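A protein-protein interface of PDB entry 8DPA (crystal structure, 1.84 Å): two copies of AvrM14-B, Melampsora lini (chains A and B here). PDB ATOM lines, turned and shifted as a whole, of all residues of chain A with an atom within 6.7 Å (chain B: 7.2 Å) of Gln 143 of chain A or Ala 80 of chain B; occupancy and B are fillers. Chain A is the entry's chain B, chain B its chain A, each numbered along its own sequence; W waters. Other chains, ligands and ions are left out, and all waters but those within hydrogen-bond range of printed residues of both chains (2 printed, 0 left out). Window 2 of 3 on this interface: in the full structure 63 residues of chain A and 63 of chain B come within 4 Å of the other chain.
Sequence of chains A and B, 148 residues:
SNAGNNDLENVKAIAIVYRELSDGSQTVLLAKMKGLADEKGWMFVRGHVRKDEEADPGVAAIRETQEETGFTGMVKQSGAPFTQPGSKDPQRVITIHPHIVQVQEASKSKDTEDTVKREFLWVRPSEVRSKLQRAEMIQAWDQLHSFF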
ATOM      1  N   ILE A 138       6.219  14.282   1.188  1.00  0.00           N
ATOM      2  CA  ILE A 138       6.886  13.920   2.439  1.00  0.00           C
ATOM      3  C   ILE A 138       6.862  15.088   3.417  1.00  0.00           C
ATOM      4  O   ILE A 138       6.647  14.903   4.623  1.00  0.00           O
ATOM      5  CB  ILE A 138       8.323  13.435   2.157  1.00  0.00           C
ATOM      6  CG1 ILE A 138       8.287  12.107   1.386  1.00  0.00           C
ATOM      7  CG2 ILE A 138       9.129  13.315   3.466  1.00  0.00           C
ATOM      8  CD1 ILE A 138       9.581  11.777   0.594  1.00  0.00           C
ATOM      9  N   GLN A 139       7.082  16.310   2.919  1.00  0.00           N
ATOM     10  CA  GLN A 139       7.027  17.470   3.798  1.00  0.00           C
ATOM     11  C   GLN A 139       5.629  17.654   4.394  1.00  0.00           C
ATOM     12  O   GLN A 139       5.492  17.908   5.597  1.00  0.00           O
ATOM     13  CB  GLN A 139       7.472  18.726   3.041  1.00  0.00           C
ATOM     14  CG  GLN A 139       7.389  20.008   3.881  1.00  0.00           C
ATOM     15  CD  GLN A 139       8.455  20.059   4.964  1.00  0.00           C
ATOM     16  OE1 GLN A 139       9.473  19.369   4.882  1.00  0.00           O
ATOM     17  NE2 GLN A 139       8.213  20.854   5.994  1.00  0.00           N
ATOM     18  N   ALA A 140       4.580  17.525   3.575  1.00  0.00           N
ATOM     19  CA  ALA A 140       3.227  17.657   4.108  1.00  0.00           C
ATOM     20  C   ALA A 140       2.989  16.630   5.209  1.00  0.00           C
ATOM     21  O   ALA A 140       2.486  16.959   6.286  1.00  0.00           O
ATOM     22  CB  ALA A 140       2.189  17.496   2.990  1.00  0.00           C
ATOM     23  N   TRP A 141       3.396  15.385   4.961  1.00  0.00           N
ATOM     24  CA  TRP A 141       3.196  14.322   5.939  1.00  0.00           C
ATOM     25  C   TRP A 141       4.034  14.560   7.190  1.00  0.00           C
ATOM     26  O   TRP A 141       3.560  14.334   8.309  1.00  0.00           O
ATOM     27  CB  TRP A 141       3.540  12.973   5.308  1.00  0.00           C
ATOM     28  CG  TRP A 141       3.316  11.798   6.211  1.00  0.00           C
ATOM     29  CD1 TRP A 141       4.273  11.004   6.782  1.00  0.00           C
ATOM     30  CD2 TRP A 141       2.048  11.266   6.627  1.00  0.00           C
ATOM     31  NE1 TRP A 141       3.675  10.010   7.531  1.00  0.00           N
ATOM     32  CE2 TRP A 141       2.312  10.148   7.453  1.00  0.00           C
ATOM     33  CE3 TRP A 141       0.719  11.630   6.386  1.00  0.00           C
ATOM     34  CZ2 TRP A 141       1.285   9.379   8.045  1.00  0.00           C
ATOM     35  CZ3 TRP A 141      -0.307  10.862   6.975  1.00  0.00           C
ATOM     36  CH2 TRP A 141      -0.012   9.751   7.794  1.00  0.00           C
ATOM     37  N   ASP A 142       5.283  15.029   7.024  1.00  0.00           N
ATOM     38  CA  ASP A 142       6.115  15.299   8.193  1.00  0.00           C
ATOM     39  C   ASP A 142       5.478  16.352   9.093  1.00  0.00           C
ATOM     40  O   ASP A 142       5.596  16.272  10.321  1.00  0.00           O
ATOM     41  CB  ASP A 142       7.523  15.750   7.768  1.00  0.00           C
ATOM     42  CG  ASP A 142       8.392  14.591   7.254  1.00  0.00           C
ATOM     43  OD1 ASP A 142       8.042  13.411   7.486  1.00  0.00           O
ATOM     44  OD2 ASP A 142       9.409  14.871   6.572  1.00  0.00           O
ATOM     45  N   GLN A 143       4.780  17.333   8.512  1.00  0.00           N
ATOM     46  CA  GLN A 143       4.184  18.369   9.350  1.00  0.00           C
ATOM     47  C   GLN A 143       2.926  17.887  10.055  1.00  0.00           C
ATOM     48  O   GLN A 143       2.630  18.357  11.158  1.00  0.00           O
ATOM     49  CB  GLN A 143       3.867  19.629   8.528  1.00  0.00           C
ATOM     50  CG  GLN A 143       5.125  20.365   8.058  1.00  0.00           C
ATOM     51  CD  GLN A 143       4.821  21.682   7.331  1.00  0.00           C
ATOM     52  OE1 GLN A 143       5.602  22.112   6.486  1.00  0.00           O
ATOM     53  NE2 GLN A 143       3.693  22.335   7.678  1.00  0.00           N
ATOM     54  N   LEU A 144       2.178  16.952   9.458  1.00  0.00           N
ATOM     55  CA  LEU A 144       0.843  16.654   9.948  1.00  0.00           C
ATOM     56  C   LEU A 144       0.649  15.224  10.442  1.00  0.00           C
ATOM     57  O   LEU A 144      -0.411  14.936  11.010  1.00  0.00           O
ATOM     58  CB  LEU A 144      -0.200  16.950   8.850  1.00  0.00           C
ATOM     59  CG  LEU A 144      -0.316  18.441   8.505  1.00  0.00           C
ATOM     60  CD1 LEU A 144      -1.098  18.679   7.239  1.00  0.00           C
ATOM     61  CD2 LEU A 144      -0.915  19.248   9.683  1.00  0.00           C
ATOM     62  N   HIS A 145       1.635  14.330  10.282  1.00  0.00           N
ATOM     63  CA  HIS A 145       1.396  12.917  10.590  1.00  0.00           C
ATOM     64  C   HIS A 145       1.020  12.673  12.050  1.00  0.00           C
ATOM     65  O   HIS A 145       0.390  11.652  12.348  1.00  0.00           O
ATOM     66  CB  HIS A 145       2.621  12.055  10.250  1.00  0.00           C
ATOM     67  CG  HIS A 145       3.773  12.243  11.187  1.00  0.00           C
ATOM     68  ND1 HIS A 145       4.096  11.326  12.163  1.00  0.00           N
ATOM     69  CD2 HIS A 145       4.677  13.247  11.300  1.00  0.00           C
ATOM     70  CE1 HIS A 145       5.148  11.756  12.839  1.00  0.00           C
ATOM     71  NE2 HIS A 145       5.520  12.921  12.336  1.00  0.00           N
ATOM     72  N   SER A 146       1.393  13.559  12.977  1.00  0.00           N
ATOM     73  CA  SER A 146       1.084  13.261  14.373  1.00  0.00           C
ATOM     74  C   SER A 146      -0.392  13.463  14.708  1.00  0.00           C
ATOM     75  O   SER A 146      -0.807  13.174  15.833  1.00  0.00           O
ATOM     76  CB  SER A 146       1.986  14.083  15.307  1.00  0.00           C
ATOM     77  OG  SER A 146       1.715  15.469  15.225  1.00  0.00           O
ATOM     78  N   PHE A 147      -1.199  13.937  13.765  1.00  0.00           N
ATOM     79  CA  PHE A 147      -2.642  13.894  13.945  1.00  0.00           C
ATOM     80  C   PHE A 147      -3.130  12.447  14.109  1.00  0.00           C
ATOM     81  O   PHE A 147      -4.063  12.189  14.879  1.00  0.00           O
ATOM     82  CB  PHE A 147      -3.318  14.555  12.743  1.00  0.00           C
ATOM     83  CG  PHE A 147      -4.817  14.414  12.732  1.00  0.00           C
ATOM     84  CD1 PHE A 147      -5.435  13.293  12.157  1.00  0.00           C
ATOM     85  CD2 PHE A 147      -5.615  15.410  13.295  1.00  0.00           C
ATOM     86  CE1 PHE A 147      -6.807  13.174  12.153  1.00  0.00           C
ATOM     87  CE2 PHE A 147      -7.005  15.291  13.294  1.00  0.00           C
ATOM     88  CZ  PHE A 147      -7.599  14.168  12.724  1.00  0.00           C
ATOM     89  N   ILE B  16      -4.588  15.939   2.904  1.00  0.00           N
ATOM     90  CA  ILE B  16      -4.425  14.562   3.359  1.00  0.00           C
ATOM     91  C   ILE B  16      -5.813  14.091   3.784  1.00  0.00           C
ATOM     92  O   ILE B  16      -6.320  14.469   4.844  1.00  0.00           O
ATOM     93  CB  ILE B  16      -3.417  14.462   4.502  1.00  0.00           C
ATOM     94  CG1 ILE B  16      -2.074  15.049   4.059  1.00  0.00           C
ATOM     95  CG2 ILE B  16      -3.250  12.996   4.948  1.00  0.00           C
ATOM     96  CD1 ILE B  16      -1.067  15.213   5.226  1.00  0.00           C
ATOM     97  N   GLN B  77      -7.134  19.985  10.615  1.00  0.00           N
ATOM     98  CA  GLN B  77      -5.831  20.511  11.009  1.00  0.00           C
ATOM     99  C   GLN B  77      -5.163  21.065   9.762  1.00  0.00           C
ATOM    100  O   GLN B  77      -5.377  20.565   8.654  1.00  0.00           O
ATOM    101  CB  GLN B  77      -4.924  19.442  11.654  1.00  0.00           C
ATOM    102  CG  GLN B  77      -3.636  20.034  12.306  1.00  0.00           C
ATOM    103  CD  GLN B  77      -2.870  19.040  13.140  1.00  0.00           C
ATOM    104  OE1 GLN B  77      -3.453  18.133  13.736  1.00  0.00           O
ATOM    105  NE2 GLN B  77      -1.562  19.230  13.229  1.00  0.00           N
ATOM    106  N   SER B  78      -4.342  22.090   9.941  1.00  0.00           N
ATOM    107  CA  SER B  78      -3.620  22.604   8.788  1.00  0.00           C
ATOM    108  C   SER B  78      -2.234  23.037   9.237  1.00  0.00           C
ATOM    109  O   SER B  78      -2.071  23.602  10.319  1.00  0.00           O
ATOM    110  CB  SER B  78      -4.380  23.745   8.120  1.00  0.00           C
ATOM    111  OG  SER B  78      -4.323  24.907   8.908  1.00  0.00           O
ATOM    112  N   GLY B  79      -1.237  22.706   8.428  1.00  0.00           N
ATOM    113  CA  GLY B  79       0.138  22.917   8.813  1.00  0.00           C
ATOM    114  C   GLY B  79       0.601  24.255   8.337  1.00  0.00           C
ATOM    115  O   GLY B  79      -0.052  24.857   7.477  1.00  0.00           O
ATOM    116  N   ALA B  80       1.706  24.727   8.907  1.00  0.00           N
ATOM    117  CA  ALA B  80       2.241  25.994   8.441  1.00  0.00           C
ATOM    118  C   ALA B  80       2.582  25.868   6.956  1.00  0.00           C
ATOM    119  O   ALA B  80       2.866  24.764   6.470  1.00  0.00           O
ATOM    120  CB  ALA B  80       3.477  26.392   9.256  1.00  0.00           C
ATOM    121  N   PRO B  81       2.505  26.966   6.197  1.00  0.00           N
ATOM    122  CA  PRO B  81       2.868  26.906   4.776  1.00  0.00           C
ATOM    123  C   PRO B  81       4.322  26.481   4.605  1.00  0.00           C
ATOM    124  O   PRO B  81       5.171  26.748   5.456  1.00  0.00           O
ATOM    125  CB  PRO B  81       2.651  28.348   4.285  1.00  0.00           C
ATOM    126  CG  PRO B  81       1.809  29.022   5.340  1.00  0.00           C
ATOM    127  CD  PRO B  81       2.131  28.324   6.631  1.00  0.00           C
ATOM    128  N   PHE B  82       4.612  25.804   3.497  1.00  0.00           N
ATOM    129  CA  PHE B  82       5.998  25.490   3.163  1.00  0.00           C
ATOM    130  C   PHE B  82       6.220  25.763   1.688  1.00  0.00           C
ATOM    131  O   PHE B  82       5.268  25.884   0.910  1.00  0.00           O
ATOM    132  CB  PHE B  82       6.404  24.041   3.529  1.00  0.00           C
ATOM    133  CG  PHE B  82       5.647  22.937   2.790  1.00  0.00           C
ATOM    134  CD1 PHE B  82       4.460  22.412   3.307  1.00  0.00           C
ATOM    135  CD2 PHE B  82       6.167  22.381   1.618  1.00  0.00           C
ATOM    136  CE1 PHE B  82       3.776  21.355   2.639  1.00  0.00           C
ATOM    137  CE2 PHE B  82       5.507  21.337   0.939  1.00  0.00           C
ATOM    138  CZ  PHE B  82       4.311  20.813   1.454  1.00  0.00           C
ATOM    139  N   THR B  83       7.497  25.883   1.315  1.00  0.00           N
ATOM    140  CA  THR B  83       7.896  26.303  -0.017  1.00  0.00           C
ATOM    141  C   THR B  83       8.615  25.182  -0.756  1.00  0.00           C
ATOM    142  O   THR B  83       9.409  24.451  -0.163  1.00  0.00           O
ATOM    143  CB  THR B  83       8.801  27.531   0.094  1.00  0.00           C
ATOM    144  OG1 THR B  83       8.057  28.573   0.722  1.00  0.00           O
ATOM    145  CG2 THR B  83       9.163  27.979  -1.210  1.00  0.00           C
ATOM    146  N   ILE B  96       2.863  26.068  -0.437  1.00  0.00           N
ATOM    147  CA  ILE B  96       1.936  24.946  -0.273  1.00  0.00           C
ATOM    148  C   ILE B  96       1.355  24.993   1.127  1.00  0.00           C
ATOM    149  O   ILE B  96       2.099  25.138   2.104  1.00  0.00           O
ATOM    150  CB  ILE B  96       2.649  23.618  -0.542  1.00  0.00           C
ATOM    151  CG1 ILE B  96       3.098  23.635  -2.004  1.00  0.00           C
ATOM    152  CG2 ILE B  96       1.743  22.429  -0.222  1.00  0.00           C
ATOM    153  CD1 ILE B  96       4.391  23.004  -2.229  1.00  0.00           C
ATOM    154  N   HIS B  97       0.024  24.887   1.218  1.00  0.00           N
ATOM    155  CA  HIS B  97      -0.709  24.891   2.481  1.00  0.00           C
ATOM    156  C   HIS B  97      -1.288  23.491   2.686  1.00  0.00           C
ATOM    157  O   HIS B  97      -2.266  23.115   2.014  1.00  0.00           O
ATOM    158  CB  HIS B  97      -1.826  25.941   2.460  1.00  0.00           C
ATOM    159  CG  HIS B  97      -1.345  27.343   2.217  1.00  0.00           C
ATOM    160  ND1 HIS B  97      -1.038  28.212   3.238  1.00  0.00           N
ATOM    161  CD2 HIS B  97      -1.139  28.030   1.067  1.00  0.00           C
ATOM    162  CE1 HIS B  97      -0.650  29.376   2.732  1.00  0.00           C
ATOM    163  NE2 HIS B  97      -0.703  29.294   1.413  1.00  0.00           N
ATOM    164  N   PRO B  98      -0.712  22.679   3.573  1.00  0.00           N
ATOM    165  CA  PRO B  98      -1.194  21.308   3.769  1.00  0.00           C
ATOM    166  C   PRO B  98      -2.264  21.207   4.850  1.00  0.00           C
ATOM    167  O   PRO B  98      -2.257  21.935   5.843  1.00  0.00           O
ATOM    168  CB  PRO B  98       0.083  20.572   4.192  1.00  0.00           C
ATOM    169  CG  PRO B  98       0.820  21.621   5.038  1.00  0.00           C
ATOM    170  CD  PRO B  98       0.463  22.984   4.413  1.00  0.00           C
HETATM  171  O   HOH W   1       6.583  24.837   6.936  1.00  0.00           O
HETATM  172  O   HOH W   2       2.880  22.568  10.527  1.00  0.00           O
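The side-chain amide oxygen (OE1) of Gln 143 of chain A sits at hydrogen-bond distance from the side-chain amide nitrogen (NE2) of Gln 139 of chain A, 2.9 Å away.
O of Phe 82 of chain B sits at hydrogen-bond distance from N of Ile 96 of chain B (2.8 Å).
The backbone carbonyl oxygen (O) of Pro 98 of chain B lies within hydrogen-bond range of the backbone NH (N) of Gly 79 of chain B (2.9 Å).
No position is printed for both chains.
The side-chain amide nitrogen of Gln 143 of chain A sits at hydrogen-bond distance from the backbone carbonyl oxygen of Ala 80 of chain B, at 2.8 Å.
Of the 10 printed residues of chain A, 5 touch a printed residue of chain B.
Hydrophobic or aromatic side chains of chain A that line the printed part of chain B: Ala 140, Leu 144 and Phe 147.
Among the printed residues, 11 pairs touch across the chains.
Among the printed residues, no Asp or Glu carboxylate lies within 4 Å of a Lys or Arg side-chain nitrogen of the other chain.
Water W1 bridges O of Pro 81 of chain B (2.8 Å) and OE1 of Gln 143 of chain A (2.9 Å).
Water W2 bridges N of Ala 80 of chain B (2.9 Å) and NE2 of Gln 143 of chain A (3.0 Å).
Of the printed residues of chain B, Ala 140 of chain A touches Phe 82 and Pro 98.
Printed residues of chain B within 4 Å of Gln 143 of chain A: Gly 79, Ala 80, Phe 82 and Pro 98.
Ala 80 of chain B touches just one residue of chain A: Gln 143.
Of the printed residues of chain A, Pro 98 of chain B touches Ala 140, Gln 143 and Leu 144.
The nearest printed residue of chain A that does not touch Gln 77 of chain B is Gln 143 of chain A (4.8 Å).
CG of Gln 139 of chain A touches CD2 of Phe 82 of chain B (3.5 Å).
Ala 140 of chain A touches Phe 82 of chain B.
Pro 98 of chain B touches Ala 140 of chain A (CB to CB, 3.9 Å).
NE2 of Gln 143 of chain A touches C of Gly 79 of chain B (3.7 Å).
Gln 143 of chain A touches Phe 82 of chain B.
Gln 143 of chain A touches Pro 98 of chain B (NE2 to CG, 3.97 Å).
Leu 144 of chain A touches Gln 77 of chain B (CD2 to NE2, 3.6 Å).
Gly 79 of chain B touches Leu 144 of chain A.
Leu 144 of chain A touches Pro 98 of chain B.
OE1 of Gln 77 of chain B touches CD2 of Phe 147 of chain A, 3.5 Å away.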
